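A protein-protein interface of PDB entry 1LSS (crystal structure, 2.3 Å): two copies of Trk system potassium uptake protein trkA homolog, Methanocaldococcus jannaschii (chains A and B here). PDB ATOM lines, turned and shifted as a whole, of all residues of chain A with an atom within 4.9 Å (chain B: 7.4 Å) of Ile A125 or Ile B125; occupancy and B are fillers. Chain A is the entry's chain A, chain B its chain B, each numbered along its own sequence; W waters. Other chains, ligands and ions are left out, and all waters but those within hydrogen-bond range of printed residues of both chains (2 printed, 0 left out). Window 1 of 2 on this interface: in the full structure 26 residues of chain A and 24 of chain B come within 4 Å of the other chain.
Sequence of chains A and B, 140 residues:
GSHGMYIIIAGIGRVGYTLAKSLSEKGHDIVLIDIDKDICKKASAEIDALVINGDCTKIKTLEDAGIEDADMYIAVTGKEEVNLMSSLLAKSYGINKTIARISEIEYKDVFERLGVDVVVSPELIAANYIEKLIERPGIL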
ATOM      1  N   VAL A 120     -33.759  21.755 -21.456  1.00  0.00           N
ATOM      2  CA  VAL A 120     -32.471  21.091 -21.572  1.00  0.00           C
ATOM      3  C   VAL A 120     -32.522  19.571 -21.459  1.00  0.00           C
ATOM      4  O   VAL A 120     -33.020  19.023 -20.480  1.00  0.00           O
ATOM      5  CB  VAL A 120     -31.486  21.623 -20.505  1.00  0.00           C
ATOM      6  CG1 VAL A 120     -30.266  20.707 -20.406  1.00  0.00           C
ATOM      7  CG2 VAL A 120     -31.054  23.020 -20.869  1.00  0.00           C
ATOM      8  N   SER A 121     -31.999  18.897 -22.475  1.00  0.00           N
ATOM      9  CA  SER A 121     -31.941  17.445 -22.468  1.00  0.00           C
ATOM     10  C   SER A 121     -30.463  17.082 -22.450  1.00  0.00           C
ATOM     11  O   SER A 121     -29.796  17.153 -23.480  1.00  0.00           O
ATOM     12  CB  SER A 121     -32.603  16.857 -23.716  1.00  0.00           C
ATOM     13  OG  SER A 121     -32.317  15.470 -23.825  1.00  0.00           O
ATOM     14  N   PRO A 122     -29.924  16.716 -21.276  1.00  0.00           N
ATOM     15  CA  PRO A 122     -28.498  16.360 -21.231  1.00  0.00           C
ATOM     16  C   PRO A 122     -28.132  15.202 -22.160  1.00  0.00           C
ATOM     17  O   PRO A 122     -27.011  15.145 -22.683  1.00  0.00           O
ATOM     18  CB  PRO A 122     -28.245  16.050 -19.750  1.00  0.00           C
ATOM     19  CG  PRO A 122     -29.622  15.823 -19.158  1.00  0.00           C
ATOM     20  CD  PRO A 122     -30.532  16.723 -19.933  1.00  0.00           C
ATOM     21  N   GLU A 123     -29.080  14.293 -22.380  1.00  0.00           N
ATOM     22  CA  GLU A 123     -28.839  13.157 -23.260  1.00  0.00           C
ATOM     23  C   GLU A 123     -28.662  13.683 -24.684  1.00  0.00           C
ATOM     24  O   GLU A 123     -27.756  13.265 -25.397  1.00  0.00           O
ATOM     25  CB  GLU A 123     -30.006  12.163 -23.206  1.00  0.00           C
ATOM     26  CG  GLU A 123     -30.174  11.425 -21.891  1.00  0.00           C
ATOM     27  CD  GLU A 123     -30.468  12.362 -20.734  1.00  0.00           C
ATOM     28  OE1 GLU A 123     -31.261  13.310 -20.925  1.00  0.00           O
ATOM     29  OE2 GLU A 123     -29.916  12.149 -19.635  1.00  0.00           O
ATOM     30  N   LEU A 124     -29.515  14.615 -25.096  1.00  0.00           N
ATOM     31  CA  LEU A 124     -29.397  15.169 -26.441  1.00  0.00           C
ATOM     32  C   LEU A 124     -28.136  16.005 -26.572  1.00  0.00           C
ATOM     33  O   LEU A 124     -27.456  15.968 -27.603  1.00  0.00           O
ATOM     34  CB  LEU A 124     -30.611  16.027 -26.790  1.00  0.00           C
ATOM     35  CG  LEU A 124     -31.904  15.259 -27.045  1.00  0.00           C
ATOM     36  CD1 LEU A 124     -33.008  16.237 -27.416  1.00  0.00           C
ATOM     37  CD2 LEU A 124     -31.682  14.239 -28.159  1.00  0.00           C
ATOM     38  N   ILE A 125     -27.826  16.766 -25.530  1.00  0.00           N
ATOM     39  CA  ILE A 125     -26.639  17.596 -25.554  1.00  0.00           C
ATOM     40  C   ILE A 125     -25.413  16.697 -25.690  1.00  0.00           C
ATOM     41  O   ILE A 125     -24.465  17.029 -26.397  1.00  0.00           O
ATOM     42  CB  ILE A 125     -26.530  18.434 -24.270  1.00  0.00           C
ATOM     43  CG1 ILE A 125     -27.694  19.423 -24.201  1.00  0.00           C
ATOM     44  CG2 ILE A 125     -25.220  19.194 -24.252  1.00  0.00           C
ATOM     45  CD1 ILE A 125     -27.697  20.276 -22.941  1.00  0.00           C
ATOM     46  N   ALA A 126     -25.444  15.558 -25.010  1.00  0.00           N
ATOM     47  CA  ALA A 126     -24.336  14.610 -25.060  1.00  0.00           C
ATOM     48  C   ALA A 126     -24.148  14.044 -26.476  1.00  0.00           C
ATOM     49  O   ALA A 126     -23.023  13.954 -26.974  1.00  0.00           O
ATOM     50  CB  ALA A 126     -24.585  13.478 -24.091  1.00  0.00           C
ATOM     51  N   ALA A 127     -25.249  13.655 -27.110  1.00  0.00           N
ATOM     52  CA  ALA A 127     -25.190  13.100 -28.456  1.00  0.00           C
ATOM     53  C   ALA A 127     -24.596  14.138 -29.397  1.00  0.00           C
ATOM     54  O   ALA A 127     -23.620  13.861 -30.086  1.00  0.00           O
ATOM     55  CB  ALA A 127     -26.593  12.685 -28.923  1.00  0.00           C
ATOM     56  N   ASN A 128     -25.172  15.340 -29.406  1.00  0.00           N
ATOM     57  CA  ASN A 128     -24.676  16.414 -30.264  1.00  0.00           C
ATOM     58  C   ASN A 128     -23.203  16.682 -30.024  1.00  0.00           C
ATOM     59  O   ASN A 128     -22.437  16.956 -30.956  1.00  0.00           O
ATOM     60  CB  ASN A 128     -25.458  17.703 -30.026  1.00  0.00           C
ATOM     61  CG  ASN A 128     -26.872  17.637 -30.575  1.00  0.00           C
ATOM     62  OD1 ASN A 128     -27.091  17.150 -31.685  1.00  0.00           O
ATOM     63  ND2 ASN A 128     -27.838  18.144 -29.808  1.00  0.00           N
ATOM     64  N   TYR A 129     -22.813  16.618 -28.759  1.00  0.00           N
ATOM     65  CA  TYR A 129     -21.433  16.855 -28.369  1.00  0.00           C
ATOM     66  C   TYR A 129     -20.529  15.813 -29.022  1.00  0.00           C
ATOM     67  O   TYR A 129     -19.454  16.131 -29.535  1.00  0.00           O
ATOM     68  CB  TYR A 129     -21.316  16.763 -26.853  1.00  0.00           C
ATOM     69  CG  TYR A 129     -19.914  16.889 -26.322  1.00  0.00           C
ATOM     70  CD1 TYR A 129     -19.400  18.128 -25.954  1.00  0.00           C
ATOM     71  CD2 TYR A 129     -19.105  15.764 -26.165  1.00  0.00           C
ATOM     72  CE1 TYR A 129     -18.112  18.247 -25.436  1.00  0.00           C
ATOM     73  CE2 TYR A 129     -17.818  15.873 -25.651  1.00  0.00           C
ATOM     74  CZ  TYR A 129     -17.330  17.117 -25.287  1.00  0.00           C
ATOM     75  OH  TYR A 129     -16.056  17.237 -24.765  1.00  0.00           O
ATOM     76  N   VAL B  15     -29.238   8.531 -25.643  1.00  0.00           N
ATOM     77  CA  VAL B  15     -28.037   9.068 -26.287  1.00  0.00           C
ATOM     78  C   VAL B  15     -27.618   8.344 -27.580  1.00  0.00           C
ATOM     79  O   VAL B  15     -27.323   8.984 -28.592  1.00  0.00           O
ATOM     80  CB  VAL B  15     -26.826   9.040 -25.321  1.00  0.00           C
ATOM     81  CG1 VAL B  15     -25.588   9.588 -26.019  1.00  0.00           C
ATOM     82  CG2 VAL B  15     -27.133   9.844 -24.070  1.00  0.00           C
ATOM     83  N   ILE B 105     -19.049  11.690 -12.495  1.00  0.00           N
ATOM     84  CA  ILE B 105     -18.071  12.642 -12.998  1.00  0.00           C
ATOM     85  C   ILE B 105     -16.692  12.515 -12.372  1.00  0.00           C
ATOM     86  O   ILE B 105     -15.691  12.756 -13.041  1.00  0.00           O
ATOM     87  CB  ILE B 105     -18.588  14.089 -12.815  1.00  0.00           C
ATOM     88  CG1 ILE B 105     -19.986  14.215 -13.442  1.00  0.00           C
ATOM     89  CG2 ILE B 105     -17.628  15.079 -13.477  1.00  0.00           C
ATOM     90  CD1 ILE B 105     -20.714  15.516 -13.115  1.00  0.00           C
ATOM     91  N   LYS B 108     -14.029  10.564 -14.359  1.00  0.00           N
ATOM     92  CA  LYS B 108     -13.688  11.014 -15.708  1.00  0.00           C
ATOM     93  C   LYS B 108     -12.189  10.892 -16.009  1.00  0.00           C
ATOM     94  O   LYS B 108     -11.799  10.287 -17.010  1.00  0.00           O
ATOM     95  CB  LYS B 108     -14.150  12.463 -15.913  1.00  0.00           C
ATOM     96  CG  LYS B 108     -13.882  13.027 -17.308  1.00  0.00           C
ATOM     97  CD  LYS B 108     -14.511  14.422 -17.478  1.00  0.00           C
ATOM     98  CE  LYS B 108     -14.409  14.942 -18.916  1.00  0.00           C
ATOM     99  NZ  LYS B 108     -13.003  15.254 -19.354  1.00  0.00           N
ATOM    100  N   VAL B 119     -14.090  10.972 -22.736  1.00  0.00           N
ATOM    101  CA  VAL B 119     -15.064  10.585 -21.725  1.00  0.00           C
ATOM    102  C   VAL B 119     -16.202  11.603 -21.736  1.00  0.00           C
ATOM    103  O   VAL B 119     -15.979  12.804 -21.643  1.00  0.00           O
ATOM    104  CB  VAL B 119     -14.431  10.534 -20.330  1.00  0.00           C
ATOM    105  CG1 VAL B 119     -15.462  10.026 -19.323  1.00  0.00           C
ATOM    106  CG2 VAL B 119     -13.188   9.631 -20.350  1.00  0.00           C
ATOM    107  N   VAL B 120     -17.430  11.121 -21.844  1.00  0.00           N
ATOM    108  CA  VAL B 120     -18.563  12.024 -21.903  1.00  0.00           C
ATOM    109  C   VAL B 120     -19.578  11.889 -20.771  1.00  0.00           C
ATOM    110  O   VAL B 120     -20.179  10.828 -20.568  1.00  0.00           O
ATOM    111  CB  VAL B 120     -19.284  11.874 -23.266  1.00  0.00           C
ATOM    112  CG1 VAL B 120     -19.489  10.398 -23.582  1.00  0.00           C
ATOM    113  CG2 VAL B 120     -20.621  12.613 -23.240  1.00  0.00           C
ATOM    114  N   SER B 121     -19.753  12.976 -20.024  1.00  0.00           N
ATOM    115  CA  SER B 121     -20.723  13.003 -18.943  1.00  0.00           C
ATOM    116  C   SER B 121     -21.868  13.881 -19.392  1.00  0.00           C
ATOM    117  O   SER B 121     -21.722  15.101 -19.467  1.00  0.00           O
ATOM    118  CB  SER B 121     -20.125  13.596 -17.667  1.00  0.00           C
ATOM    119  OG  SER B 121     -21.169  14.017 -16.793  1.00  0.00           O
ATOM    120  N   PRO B 122     -23.030  13.281 -19.685  1.00  0.00           N
ATOM    121  CA  PRO B 122     -24.171  14.091 -20.124  1.00  0.00           C
ATOM    122  C   PRO B 122     -24.518  15.190 -19.110  1.00  0.00           C
ATOM    123  O   PRO B 122     -24.886  16.309 -19.488  1.00  0.00           O
ATOM    124  CB  PRO B 122     -25.287  13.057 -20.281  1.00  0.00           C
ATOM    125  CG  PRO B 122     -24.534  11.784 -20.609  1.00  0.00           C
ATOM    126  CD  PRO B 122     -23.378  11.851 -19.645  1.00  0.00           C
ATOM    127  N   GLU B 123     -24.387  14.876 -17.825  1.00  0.00           N
ATOM    128  CA  GLU B 123     -24.697  15.849 -16.772  1.00  0.00           C
ATOM    129  C   GLU B 123     -23.696  17.003 -16.704  1.00  0.00           C
ATOM    130  O   GLU B 123     -24.085  18.167 -16.599  1.00  0.00           O
ATOM    131  CB  GLU B 123     -24.790  15.157 -15.411  1.00  0.00           C
ATOM    132  CG  GLU B 123     -25.997  14.231 -15.238  1.00  0.00           C
ATOM    133  CD  GLU B 123     -25.913  12.972 -16.084  1.00  0.00           C
ATOM    134  OE1 GLU B 123     -24.796  12.437 -16.246  1.00  0.00           O
ATOM    135  OE2 GLU B 123     -26.962  12.506 -16.578  1.00  0.00           O
ATOM    136  N   LEU B 124     -22.407  16.694 -16.747  1.00  0.00           N
ATOM    137  CA  LEU B 124     -21.388  17.742 -16.719  1.00  0.00           C
ATOM    138  C   LEU B 124     -21.549  18.641 -17.962  1.00  0.00           C
ATOM    139  O   LEU B 124     -21.605  19.872 -17.855  1.00  0.00           O
ATOM    140  CB  LEU B 124     -19.991  17.101 -16.688  1.00  0.00           C
ATOM    141  CG  LEU B 124     -18.726  17.974 -16.609  1.00  0.00           C
ATOM    142  CD1 LEU B 124     -18.423  18.556 -17.965  1.00  0.00           C
ATOM    143  CD2 LEU B 124     -18.918  19.091 -15.564  1.00  0.00           C
ATOM    144  N   ILE B 125     -21.655  18.022 -19.136  1.00  0.00           N
ATOM    145  CA  ILE B 125     -21.806  18.760 -20.385  1.00  0.00           C
ATOM    146  C   ILE B 125     -23.051  19.639 -20.371  1.00  0.00           C
ATOM    147  O   ILE B 125     -23.027  20.755 -20.902  1.00  0.00           O
ATOM    148  CB  ILE B 125     -21.870  17.796 -21.593  1.00  0.00           C
ATOM    149  CG1 ILE B 125     -20.587  16.955 -21.646  1.00  0.00           C
ATOM    150  CG2 ILE B 125     -22.028  18.582 -22.892  1.00  0.00           C
ATOM    151  CD1 ILE B 125     -20.626  15.857 -22.675  1.00  0.00           C
ATOM    152  N   ALA B 126     -24.131  19.137 -19.766  1.00  0.00           N
ATOM    153  CA  ALA B 126     -25.380  19.903 -19.671  1.00  0.00           C
ATOM    154  C   ALA B 126     -25.216  21.086 -18.711  1.00  0.00           C
ATOM    155  O   ALA B 126     -25.795  22.147 -18.923  1.00  0.00           O
ATOM    156  CB  ALA B 126     -26.541  19.001 -19.209  1.00  0.00           C
ATOM    157  N   ALA B 127     -24.437  20.895 -17.651  1.00  0.00           N
ATOM    158  CA  ALA B 127     -24.192  21.977 -16.696  1.00  0.00           C
ATOM    159  C   ALA B 127     -23.358  23.065 -17.382  1.00  0.00           C
ATOM    160  O   ALA B 127     -23.598  24.251 -17.177  1.00  0.00           O
ATOM    161  CB  ALA B 127     -23.460  21.452 -15.460  1.00  0.00           C
ATOM    162  N   ASN B 128     -22.382  22.661 -18.195  1.00  0.00           N
ATOM    163  CA  ASN B 128     -21.548  23.626 -18.919  1.00  0.00           C
ATOM    164  C   ASN B 128     -22.405  24.387 -19.922  1.00  0.00           C
ATOM    165  O   ASN B 128     -22.271  25.599 -20.089  1.00  0.00           O
ATOM    166  CB  ASN B 128     -20.423  22.929 -19.697  1.00  0.00           C
ATOM    167  CG  ASN B 128     -19.358  22.326 -18.796  1.00  0.00           C
ATOM    168  OD1 ASN B 128     -19.102  22.820 -17.691  1.00  0.00           O
ATOM    169  ND2 ASN B 128     -18.708  21.261 -19.278  1.00  0.00           N
ATOM    170  N   TYR B 129     -23.282  23.660 -20.599  1.00  0.00           N
ATOM    171  CA  TYR B 129     -24.159  24.253 -21.594  1.00  0.00           C
ATOM    172  C   TYR B 129     -25.036  25.341 -20.988  1.00  0.00           C
ATOM    173  O   TYR B 129     -25.112  26.445 -21.518  1.00  0.00           O
ATOM    174  CB  TYR B 129     -25.040  23.179 -22.216  1.00  0.00           C
ATOM    175  CG  TYR B 129     -26.070  23.712 -23.187  1.00  0.00           C
ATOM    176  CD1 TYR B 129     -25.711  24.065 -24.491  1.00  0.00           C
ATOM    177  CD2 TYR B 129     -27.411  23.825 -22.815  1.00  0.00           C
ATOM    178  CE1 TYR B 129     -26.669  24.503 -25.406  1.00  0.00           C
ATOM    179  CE2 TYR B 129     -28.375  24.261 -23.717  1.00  0.00           C
ATOM    180  CZ  TYR B 129     -27.999  24.599 -25.011  1.00  0.00           C
ATOM    181  OH  TYR B 129     -28.950  25.020 -25.913  1.00  0.00           O
ATOM    182  N   ILE B 130     -25.701  25.020 -19.880  1.00  0.00           N
ATOM    183  CA  ILE B 130     -26.568  25.976 -19.203  1.00  0.00           C
ATOM    184  C   ILE B 130     -25.719  27.163 -18.759  1.00  0.00           C
ATOM    185  O   ILE B 130     -26.127  28.318 -18.877  1.00  0.00           O
ATOM    186  CB  ILE B 130     -27.240  25.342 -17.960  1.00  0.00           C
ATOM    187  CG1 ILE B 130     -28.281  24.311 -18.400  1.00  0.00           C
ATOM    188  CG2 ILE B 130     -27.878  26.414 -17.097  1.00  0.00           C
ATOM    189  CD1 ILE B 130     -28.939  23.560 -17.243  1.00  0.00           C
ATOM    190  N   GLU B 131     -24.527  26.868 -18.257  1.00  0.00           N
ATOM    191  CA  GLU B 131     -23.629  27.915 -17.812  1.00  0.00           C
ATOM    192  C   GLU B 131     -23.328  28.905 -18.948  1.00  0.00           C
ATOM    193  O   GLU B 131     -23.224  30.115 -18.720  1.00  0.00           O
ATOM    194  CB  GLU B 131     -22.339  27.296 -17.281  1.00  0.00           C
ATOM    195  CG  GLU B 131     -21.312  28.311 -16.838  1.00  0.00           C
ATOM    196  CD  GLU B 131     -20.108  27.660 -16.193  1.00  0.00           C
ATOM    197  OE1 GLU B 131     -19.969  26.415 -16.320  1.00  0.00           O
ATOM    198  OE2 GLU B 131     -19.301  28.393 -15.571  1.00  0.00           O
ATOM    199  N   LYS B 132     -23.213  28.406 -20.179  1.00  0.00           N
ATOM    200  CA  LYS B 132     -22.921  29.261 -21.318  1.00  0.00           C
ATOM    201  C   LYS B 132     -24.114  30.144 -21.650  1.00  0.00           C
ATOM    202  O   LYS B 132     -23.929  31.299 -22.059  1.00  0.00           O
ATOM    203  CB  LYS B 132     -22.509  28.413 -22.520  1.00  0.00           C
ATOM    204  CG  LYS B 132     -21.258  27.581 -22.283  1.00  0.00           C
ATOM    205  CD  LYS B 132     -20.769  26.941 -23.571  1.00  0.00           C
ATOM    206  CE  LYS B 132     -19.522  26.103 -23.331  1.00  0.00           C
ATOM    207  NZ  LYS B 132     -19.027  25.472 -24.584  1.00  0.00           N
HETATM  208  O   HOH W   1     -29.541  13.061 -17.125  1.00  0.00           O
HETATM  209  O   HOH W   2     -27.417  10.452 -18.797  1.00  0.00           O
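Among the printed residues, pairs that only touch across the chains: Pro A122 with Pro B122, Pro A122 with Ala B126, Ile A125 with Ile B125, Ile A125 with Tyr B129, Glu A123 with Val B15, Ala A127 with Val B15, Tyr A129 with Ile B125, Ala A126 with Pro B122 and Val A120 with Ile B130.
Ile A125 touches just these residues of chain B: Ile B125 and Tyr B129. Of chain A, only Ile A125 (3.5 Å) and Tyr A129 (3.8 Å) come within 4 Å of Ile B125. Printed residues of chain B within 4 Å of Ala A126: Pro B122. Of the printed residues of chain A, Pro B122 touches Pro A122 (3.4 Å) and Ala A126 (3.9 Å). Printed residues of chain B within 4 Å of Val A120: Ile B130. Of the printed residues of chain B, Pro A122 touches Pro B122 (3.4 Å) and Ala B126 (3.5 Å). Printed residues of chain A within 4 Å of Val B15: Glu A123 (3.7 Å) and Ala A127 (3.8 Å). Glu B123 touches none of the printed residues of chain A. The nearest residue of chain B that does not touch Ile A125 is Ala B126 (4.02 Å).
Along chain A the printed residues that touch a printed residue of chain B span positions 120 to 129. Hydrophobic or aromatic side chains of chain B that line the printed part of chain A: Val B15, Pro B122, Ile B125, Ala B126, Tyr B129 and Ile B130. Among the printed residues, no Asp or Glu carboxylate lies within 4 Å of a Lys or Arg side-chain nitrogen of the other chain.
Pro B122 touches its own counterpart, Pro A122. Pro A122 touches Ala B126, and with the chains exchanged Ala A126 touches Pro B122. Ile B125 touches its own counterpart, Ile A125. Ile A125 touches Tyr B129, and with the chains exchanged Tyr A129 touches Ile B125. Positions printed for both chains: 120, 121, 122, 123, 124, 125, 126, 127, 128 and 129. Of the 9 pairs that touch across the chains among the printed residues, 6 have their exchanged pair printed and touching as well.
Water W1 bridges the side-chain carboxylate of Glu B123 (2.7 Å) and the side-chain carboxylate of Glu A123 (2.7 Å). Water W2 lies within hydrogen-bond range of the side-chain carboxylate (OE2) of Glu B123 (3.1 Å) and the side-chain carboxylate (OE2) of Glu A123 (3.1 Å).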
